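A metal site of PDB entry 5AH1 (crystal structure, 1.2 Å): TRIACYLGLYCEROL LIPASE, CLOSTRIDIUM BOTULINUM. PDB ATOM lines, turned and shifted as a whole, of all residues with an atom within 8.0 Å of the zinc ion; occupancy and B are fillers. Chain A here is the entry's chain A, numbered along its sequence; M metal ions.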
ATOM      1  N   SER A 126     -19.637  -5.128 -19.457  1.00  0.00           N
ATOM      2  CA  SER A 126     -19.359  -5.229 -18.031  1.00  0.00           C
ATOM      3  C   SER A 126     -18.672  -6.545 -17.672  1.00  0.00           C
ATOM      4  O   SER A 126     -18.582  -7.479 -18.478  1.00  0.00           O
ATOM      5  CB  SER A 126     -20.632  -5.017 -17.229  1.00  0.00           C
ATOM      6  OG  SER A 126     -21.114  -3.702 -17.467  1.00  0.00           O
ATOM      7  N   SER A 127     -18.189  -6.642 -16.427  1.00  0.00           N
ATOM      8  CA  SER A 127     -17.531  -7.851 -15.974  1.00  0.00           C
ATOM      9  C   SER A 127     -18.522  -9.008 -15.861  1.00  0.00           C
ATOM     10  O   SER A 127     -19.727  -8.829 -15.817  1.00  0.00           O
ATOM     11  CB  SER A 127     -16.915  -7.628 -14.605  1.00  0.00           C
ATOM     12  OG  SER A 127     -17.938  -7.404 -13.657  1.00  0.00           O
ATOM     13  N   ASN A 128     -17.993 -10.226 -15.810  1.00  0.00           N
ATOM     14  CA  ASN A 128     -18.830 -11.403 -15.604  1.00  0.00           C
ATOM     15  C   ASN A 128     -19.545 -11.361 -14.243  1.00  0.00           C
ATOM     16  O   ASN A 128     -20.690 -11.787 -14.147  1.00  0.00           O
ATOM     17  CB  ASN A 128     -17.994 -12.674 -15.760  1.00  0.00           C
ATOM     18  CG  ASN A 128     -17.819 -13.040 -17.213  1.00  0.00           C
ATOM     19  OD1 ASN A 128     -18.813 -13.209 -17.929  1.00  0.00           O
ATOM     20  ND2 ASN A 128     -16.581 -13.207 -17.646  1.00  0.00           N
ATOM     21  N   TRP A 129     -18.889 -10.876 -13.208  1.00  0.00           N
ATOM     22  CA  TRP A 129     -19.569 -10.699 -11.925  1.00  0.00           C
ATOM     23  C   TRP A 129     -20.779  -9.775 -12.099  1.00  0.00           C
ATOM     24  O   TRP A 129     -21.912 -10.097 -11.701  1.00  0.00           O
ATOM     25  CB  TRP A 129     -18.620 -10.104 -10.901  1.00  0.00           C
ATOM     26  CG  TRP A 129     -19.267  -9.788  -9.576  1.00  0.00           C
ATOM     27  CD1 TRP A 129     -20.032  -8.684  -9.265  1.00  0.00           C
ATOM     28  CD2 TRP A 129     -19.208 -10.574  -8.359  1.00  0.00           C
ATOM     29  NE1 TRP A 129     -20.437  -8.739  -7.958  1.00  0.00           N
ATOM     30  CE2 TRP A 129     -19.940  -9.879  -7.377  1.00  0.00           C
ATOM     31  CE3 TRP A 129     -18.613 -11.799  -8.015  1.00  0.00           C
ATOM     32  CZ2 TRP A 129     -20.051 -10.335  -6.070  1.00  0.00           C
ATOM     33  CZ3 TRP A 129     -18.729 -12.249  -6.729  1.00  0.00           C
ATOM     34  CH2 TRP A 129     -19.451 -11.533  -5.777  1.00  0.00           C
ATOM     35  N   ASP A 130     -20.550  -8.612 -12.707  1.00  0.00           N
ATOM     36  CA  ASP A 130     -21.627  -7.633 -12.842  1.00  0.00           C
ATOM     37  C   ASP A 130     -22.751  -8.229 -13.690  1.00  0.00           C
ATOM     38  O   ASP A 130     -23.934  -8.097 -13.369  1.00  0.00           O
ATOM     39  CB  ASP A 130     -21.136  -6.321 -13.465  1.00  0.00           C
ATOM     40  CG  ASP A 130     -20.199  -5.497 -12.548  1.00  0.00           C
ATOM     41  OD1 ASP A 130     -19.817  -5.954 -11.432  1.00  0.00           O
ATOM     42  OD2 ASP A 130     -19.859  -4.367 -12.956  1.00  0.00           O
ATOM     43  N   ARG A 131     -22.380  -8.873 -14.786  1.00  0.00           N
ATOM     44  CA  ARG A 131     -23.353  -9.514 -15.661  1.00  0.00           C
ATOM     45  C   ARG A 131     -24.143 -10.622 -14.975  1.00  0.00           C
ATOM     46  O   ARG A 131     -25.318 -10.792 -15.233  1.00  0.00           O
ATOM     47  CB  ARG A 131     -22.656 -10.009 -16.925  1.00  0.00           C
ATOM     48  CG  ARG A 131     -22.211  -8.838 -17.844  1.00  0.00           C
ATOM     49  CD  ARG A 131     -21.225  -9.294 -18.895  1.00  0.00           C
ATOM     50  NE  ARG A 131     -21.591 -10.540 -19.579  1.00  0.00           N
ATOM     51  CZ  ARG A 131     -21.967 -10.633 -20.855  1.00  0.00           C
ATOM     52  NH1 ARG A 131     -22.209  -9.571 -21.619  1.00  0.00           N
ATOM     53  NH2 ARG A 131     -22.163 -11.844 -21.353  1.00  0.00           N
ATOM     54  N   CYS A 133     -24.859 -10.732 -11.711  1.00  0.00           N
ATOM     55  CA  CYS A 133     -25.798 -10.049 -10.830  1.00  0.00           C
ATOM     56  C   CYS A 133     -26.964  -9.504 -11.627  1.00  0.00           C
ATOM     57  O   CYS A 133     -28.115  -9.542 -11.176  1.00  0.00           O
ATOM     58  CB  CYS A 133     -25.093  -8.909 -10.084  1.00  0.00           C
ATOM     59  SG  CYS A 133     -23.776  -9.445  -8.943  1.00  0.00           S
ATOM     60  N   GLU A 134     -26.679  -8.958 -12.799  1.00  0.00           N
ATOM     61  CA  GLU A 134     -27.722  -8.456 -13.689  1.00  0.00           C
ATOM     62  C   GLU A 134     -28.607  -9.602 -14.167  1.00  0.00           C
ATOM     63  O   GLU A 134     -29.831  -9.450 -14.226  1.00  0.00           O
ATOM     64  CB  GLU A 134     -27.091  -7.703 -14.846  1.00  0.00           C
ATOM     65  CG  GLU A 134     -26.389  -6.429 -14.366  1.00  0.00           C
ATOM     66  CD  GLU A 134     -25.336  -5.919 -15.325  1.00  0.00           C
ATOM     67  OE1 GLU A 134     -25.187  -6.454 -16.435  1.00  0.00           O
ATOM     68  OE2 GLU A 134     -24.643  -4.941 -14.952  1.00  0.00           O
ATOM     69  N   TYR A 146     -25.001  -5.523  -6.836  1.00  0.00           N
ATOM     70  CA  TYR A 146     -23.675  -6.049  -7.158  1.00  0.00           C
ATOM     71  C   TYR A 146     -22.899  -6.520  -5.934  1.00  0.00           C
ATOM     72  O   TYR A 146     -21.805  -7.052  -6.088  1.00  0.00           O
ATOM     73  CB  TYR A 146     -22.854  -4.976  -7.890  1.00  0.00           C
ATOM     74  CG  TYR A 146     -23.438  -4.563  -9.226  1.00  0.00           C
ATOM     75  CD1 TYR A 146     -23.395  -5.432 -10.294  1.00  0.00           C
ATOM     76  CD2 TYR A 146     -24.051  -3.328  -9.401  1.00  0.00           C
ATOM     77  CE1 TYR A 146     -23.917  -5.082 -11.519  1.00  0.00           C
ATOM     78  CE2 TYR A 146     -24.574  -2.963 -10.626  1.00  0.00           C
ATOM     79  CZ  TYR A 146     -24.518  -3.845 -11.682  1.00  0.00           C
ATOM     80  OH  TYR A 146     -25.047  -3.452 -12.888  1.00  0.00           O
ATOM     81  N   GLY A 147     -23.460  -6.315  -4.747  1.00  0.00           N
ATOM     82  CA  GLY A 147     -22.811  -6.668  -3.503  1.00  0.00           C
ATOM     83  C   GLY A 147     -22.099  -5.468  -2.899  1.00  0.00           C
ATOM     84  O   GLY A 147     -21.339  -4.781  -3.571  1.00  0.00           O
ATOM     85  N   HIS A 150     -18.154  -6.050  -3.104  1.00  0.00           N
ATOM     86  CA  HIS A 150     -17.671  -5.898  -4.472  1.00  0.00           C
ATOM     87  C   HIS A 150     -17.727  -4.448  -4.914  1.00  0.00           C
ATOM     88  O   HIS A 150     -16.753  -3.924  -5.471  1.00  0.00           O
ATOM     89  CB  HIS A 150     -18.548  -6.746  -5.390  1.00  0.00           C
ATOM     90  CG  HIS A 150     -18.241  -6.555  -6.845  1.00  0.00           C
ATOM     91  ND1 HIS A 150     -17.427  -7.398  -7.559  1.00  0.00           N
ATOM     92  CD2 HIS A 150     -18.672  -5.611  -7.716  1.00  0.00           C
ATOM     93  CE1 HIS A 150     -17.363  -6.987  -8.812  1.00  0.00           C
ATOM     94  NE2 HIS A 150     -18.102  -5.887  -8.931  1.00  0.00           N
ATOM     95  N   ALA A 151     -18.845  -3.787  -4.665  1.00  0.00           N
ATOM     96  CA  ALA A 151     -19.006  -2.417  -5.131  1.00  0.00           C
ATOM     97  C   ALA A 151     -17.988  -1.494  -4.437  1.00  0.00           C
ATOM     98  O   ALA A 151     -17.452  -0.561  -5.045  1.00  0.00           O
ATOM     99  CB  ALA A 151     -20.423  -1.937  -4.891  1.00  0.00           C
ATOM    100  N   LYS A 153     -14.982  -2.491  -3.243  1.00  0.00           N
ATOM    101  CA  LYS A 153     -13.671  -2.854  -3.763  1.00  0.00           C
ATOM    102  C   LYS A 153     -13.382  -2.228  -5.118  1.00  0.00           C
ATOM    103  O   LYS A 153     -12.289  -1.706  -5.355  1.00  0.00           O
ATOM    104  CB  LYS A 153     -13.561  -4.374  -3.857  1.00  0.00           C
ATOM    105  CG  LYS A 153     -12.239  -4.873  -4.423  1.00  0.00           C
ATOM    106  CD  LYS A 153     -12.197  -6.396  -4.437  1.00  0.00           C
ATOM    107  CE  LYS A 153     -10.896  -6.903  -5.006  1.00  0.00           C
ATOM    108  NZ  LYS A 153      -9.766  -6.595  -4.070  1.00  0.00           N
ATOM    109  N   PHE A 154     -14.368  -2.282  -6.008  1.00  0.00           N
ATOM    110  CA  PHE A 154     -14.184  -1.814  -7.376  1.00  0.00           C
ATOM    111  C   PHE A 154     -14.637  -0.368  -7.602  1.00  0.00           C
ATOM    112  O   PHE A 154     -14.491   0.169  -8.694  1.00  0.00           O
ATOM    113  CB  PHE A 154     -14.825  -2.815  -8.347  1.00  0.00           C
ATOM    114  CG  PHE A 154     -14.087  -4.118  -8.406  1.00  0.00           C
ATOM    115  CD1 PHE A 154     -12.799  -4.191  -8.895  1.00  0.00           C
ATOM    116  CD2 PHE A 154     -14.675  -5.281  -7.942  1.00  0.00           C
ATOM    117  CE1 PHE A 154     -12.122  -5.393  -8.934  1.00  0.00           C
ATOM    118  CE2 PHE A 154     -13.991  -6.489  -7.979  1.00  0.00           C
ATOM    119  CZ  PHE A 154     -12.710  -6.541  -8.480  1.00  0.00           C
ATOM    120  N   LYS A 155     -15.144   0.263  -6.547  1.00  0.00           N
ATOM    121  CA  LYS A 155     -15.509   1.680  -6.568  1.00  0.00           C
ATOM    122  C   LYS A 155     -16.593   1.983  -7.590  1.00  0.00           C
ATOM    123  O   LYS A 155     -16.466   2.876  -8.419  1.00  0.00           O
ATOM    124  CB  LYS A 155     -14.280   2.548  -6.812  1.00  0.00           C
ATOM    125  CG  LYS A 155     -13.139   2.241  -5.832  1.00  0.00           C
ATOM    126  CD  LYS A 155     -11.879   3.015  -6.190  1.00  0.00           C
ATOM    127  CE  LYS A 155     -10.732   2.665  -5.229  1.00  0.00           C
ATOM    128  NZ  LYS A 155     -10.384   1.211  -5.219  1.00  0.00           N
ATOM    129  N   HIS A 156     -17.677   1.222  -7.519  1.00  0.00           N
ATOM    130  CA  HIS A 156     -18.865   1.496  -8.304  1.00  0.00           C
ATOM    131  C   HIS A 156     -20.125   1.326  -7.462  1.00  0.00           C
ATOM    132  O   HIS A 156     -20.054   0.980  -6.292  1.00  0.00           O
ATOM    133  CB  HIS A 156     -18.878   0.727  -9.644  1.00  0.00           C
ATOM    134  CG  HIS A 156     -19.171  -0.758  -9.595  1.00  0.00           C
ATOM    135  ND1 HIS A 156     -20.375  -1.298  -9.173  1.00  0.00           N
ATOM    136  CD2 HIS A 156     -18.447  -1.800 -10.065  1.00  0.00           C
ATOM    137  CE1 HIS A 156     -20.337  -2.607  -9.342  1.00  0.00           C
ATOM    138  NE2 HIS A 156     -19.195  -2.942  -9.898  1.00  0.00           N
ATOM    139  N   ASN A 157     -21.279   1.617  -8.040  1.00  0.00           N
ATOM    140  CA  ASN A 157     -22.517   1.596  -7.289  1.00  0.00           C
ATOM    141  C   ASN A 157     -22.873   0.181  -6.897  1.00  0.00           C
ATOM    142  O   ASN A 157     -22.672  -0.758  -7.677  1.00  0.00           O
ATOM    143  CB  ASN A 157     -23.671   2.133  -8.124  1.00  0.00           C
ATOM    144  CG  ASN A 157     -23.614   3.622  -8.328  1.00  0.00           C
ATOM    145  OD1 ASN A 157     -23.023   4.343  -7.540  1.00  0.00           O
ATOM    146  ND2 ASN A 157     -24.239   4.082  -9.398  1.00  0.00           N
ATOM    147  N   GLN A 273     -23.664   1.600 -13.408  1.00  0.00           N
ATOM    148  CA  GLN A 273     -23.006   1.405 -12.126  1.00  0.00           C
ATOM    149  C   GLN A 273     -21.723   2.218 -12.017  1.00  0.00           C
ATOM    150  O   GLN A 273     -21.282   2.510 -10.918  1.00  0.00           O
ATOM    151  CB  GLN A 273     -22.778  -0.085 -11.810  1.00  0.00           C
ATOM    152  CG  GLN A 273     -21.617  -0.758 -12.547  1.00  0.00           C
ATOM    153  CD  GLN A 273     -21.980  -1.203 -13.945  1.00  0.00           C
ATOM    154  OE1 GLN A 273     -22.686  -0.526 -14.688  1.00  0.00           O
ATOM    155  NE2 GLN A 273     -21.486  -2.374 -14.325  1.00  0.00           N
ATOM    156  N   TRP A 274     -21.148   2.533 -13.173  1.00  0.00           N
ATOM    157  CA  TRP A 274     -19.923   3.312 -13.285  1.00  0.00           C
ATOM    158  C   TRP A 274     -20.170   4.805 -13.472  1.00  0.00           C
ATOM    159  O   TRP A 274     -19.237   5.549 -13.686  1.00  0.00           O
ATOM    160  CB  TRP A 274     -19.087   2.796 -14.457  1.00  0.00           C
ATOM    161  CG  TRP A 274     -18.553   1.405 -14.280  1.00  0.00           C
ATOM    162  CD1 TRP A 274     -18.974   0.264 -14.904  1.00  0.00           C
ATOM    163  CD2 TRP A 274     -17.497   1.010 -13.401  1.00  0.00           C
ATOM    164  NE1 TRP A 274     -18.252  -0.813 -14.484  1.00  0.00           N
ATOM    165  CE2 TRP A 274     -17.323  -0.387 -13.570  1.00  0.00           C
ATOM    166  CE3 TRP A 274     -16.667   1.690 -12.507  1.00  0.00           C
ATOM    167  CZ2 TRP A 274     -16.365  -1.101 -12.861  1.00  0.00           C
ATOM    168  CZ3 TRP A 274     -15.714   0.982 -11.818  1.00  0.00           C
ATOM    169  CH2 TRP A 274     -15.573  -0.411 -12.002  1.00  0.00           C
ATOM    170  N   THR A 300      -9.396  -0.604 -14.216  1.00  0.00           N
ATOM    171  CA  THR A 300     -10.040  -1.603 -13.369  1.00  0.00           C
ATOM    172  C   THR A 300      -9.967  -2.987 -13.987  1.00  0.00           C
ATOM    173  O   THR A 300      -9.943  -3.131 -15.213  1.00  0.00           O
ATOM    174  CB  THR A 300     -11.536  -1.256 -13.097  1.00  0.00           C
ATOM    175  OG1 THR A 300     -12.084  -2.186 -12.157  1.00  0.00           O
ATOM    176  CG2 THR A 300     -12.388  -1.290 -14.382  1.00  0.00           C
ATOM    177  N   LYS A 301      -9.924  -4.021 -13.151  1.00  0.00           N
ATOM    178  CA  LYS A 301     -10.117  -5.375 -13.686  1.00  0.00           C
ATOM    179  C   LYS A 301     -11.600  -5.754 -13.712  1.00  0.00           C
ATOM    180  O   LYS A 301     -11.935  -6.820 -14.224  1.00  0.00           O
ATOM    181  CB  LYS A 301      -9.284  -6.395 -12.918  1.00  0.00           C
ATOM    182  CG  LYS A 301      -9.696  -6.639 -11.497  1.00  0.00           C
ATOM    183  CD  LYS A 301      -8.834  -7.756 -10.925  1.00  0.00           C
ATOM    184  CE  LYS A 301      -9.244  -8.170  -9.511  1.00  0.00           C
ATOM    185  NZ  LYS A 301      -8.302  -9.218  -8.989  1.00  0.00           N
ATOM    186  N   ASP A 302     -12.474  -4.907 -13.179  1.00  0.00           N
ATOM    187  CA  ASP A 302     -13.912  -5.210 -13.169  1.00  0.00           C
ATOM    188  C   ASP A 302     -14.628  -4.771 -14.444  1.00  0.00           C
ATOM    189  O   ASP A 302     -15.566  -3.967 -14.394  1.00  0.00           O
ATOM    190  CB  ASP A 302     -14.539  -4.562 -11.939  1.00  0.00           C
ATOM    191  CG  ASP A 302     -15.973  -4.984 -11.683  1.00  0.00           C
ATOM    192  OD1 ASP A 302     -16.314  -6.183 -11.870  1.00  0.00           O
ATOM    193  OD2 ASP A 302     -16.770  -4.113 -11.251  1.00  0.00           O
ATOM    194  N   ILE A 303     -14.177  -5.268 -15.591  1.00  0.00           N
ATOM    195  CA  ILE A 303     -14.699  -4.857 -16.898  1.00  0.00           C
ATOM    196  C   ILE A 303     -14.521  -6.017 -17.889  1.00  0.00           C
ATOM    197  O   ILE A 303     -13.681  -6.885 -17.669  1.00  0.00           O
ATOM    198  CB  ILE A 303     -13.986  -3.541 -17.327  1.00  0.00           C
ATOM    199  CG1 ILE A 303     -14.765  -2.818 -18.435  1.00  0.00           C
ATOM    200  CG2 ILE A 303     -12.536  -3.802 -17.677  1.00  0.00           C
ATOM    201  CD1 ILE A 303     -16.099  -2.246 -17.983  1.00  0.00           C
HETATM  202 ZN    ZN M   1     -18.523  -4.763 -10.632  1.00  0.00          ZN
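N of Asp 130 is in hydrogen-bond range of OG of Ser 127 (3.0 Å).
The side-chain carboxylate (OD2) of Asp 130 is in hydrogen-bond range of the side-chain amide nitrogen (NE2) of Gln 273.
The side-chain carboxylate of Asp 302 lies within hydrogen-bond range of the side-chain hydroxyl of Ser 127, at 2.7 Å.
The backbone NH (N) of Asp 302 is in hydrogen-bond range of the side-chain hydroxyl (OG1) of Thr 300 (2.9 Å).
The backbone NH (N) of His 156 sits at hydrogen-bond distance from the backbone carbonyl oxygen (O) of Ala 151 (3.1 Å).
ND1 of His 150 lies close to NE1 of Trp 129.
Of the 23 residues printed, 4 come within 4 Å of the zinc ion.
The nearest printed residue that does not touch the zinc ion is Ser 127 (4.1 Å).
The zinc ion is bound by OD1 of Asp 130, OD2 of Asp 302, NE2 of His 156 and NE2 of His 150.
The zinc ion has four donor atoms within binding distance.
Slightly farther from the zinc ion lies the side-chain carboxylate (OD2) of Asp 130 (2.7 Å).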
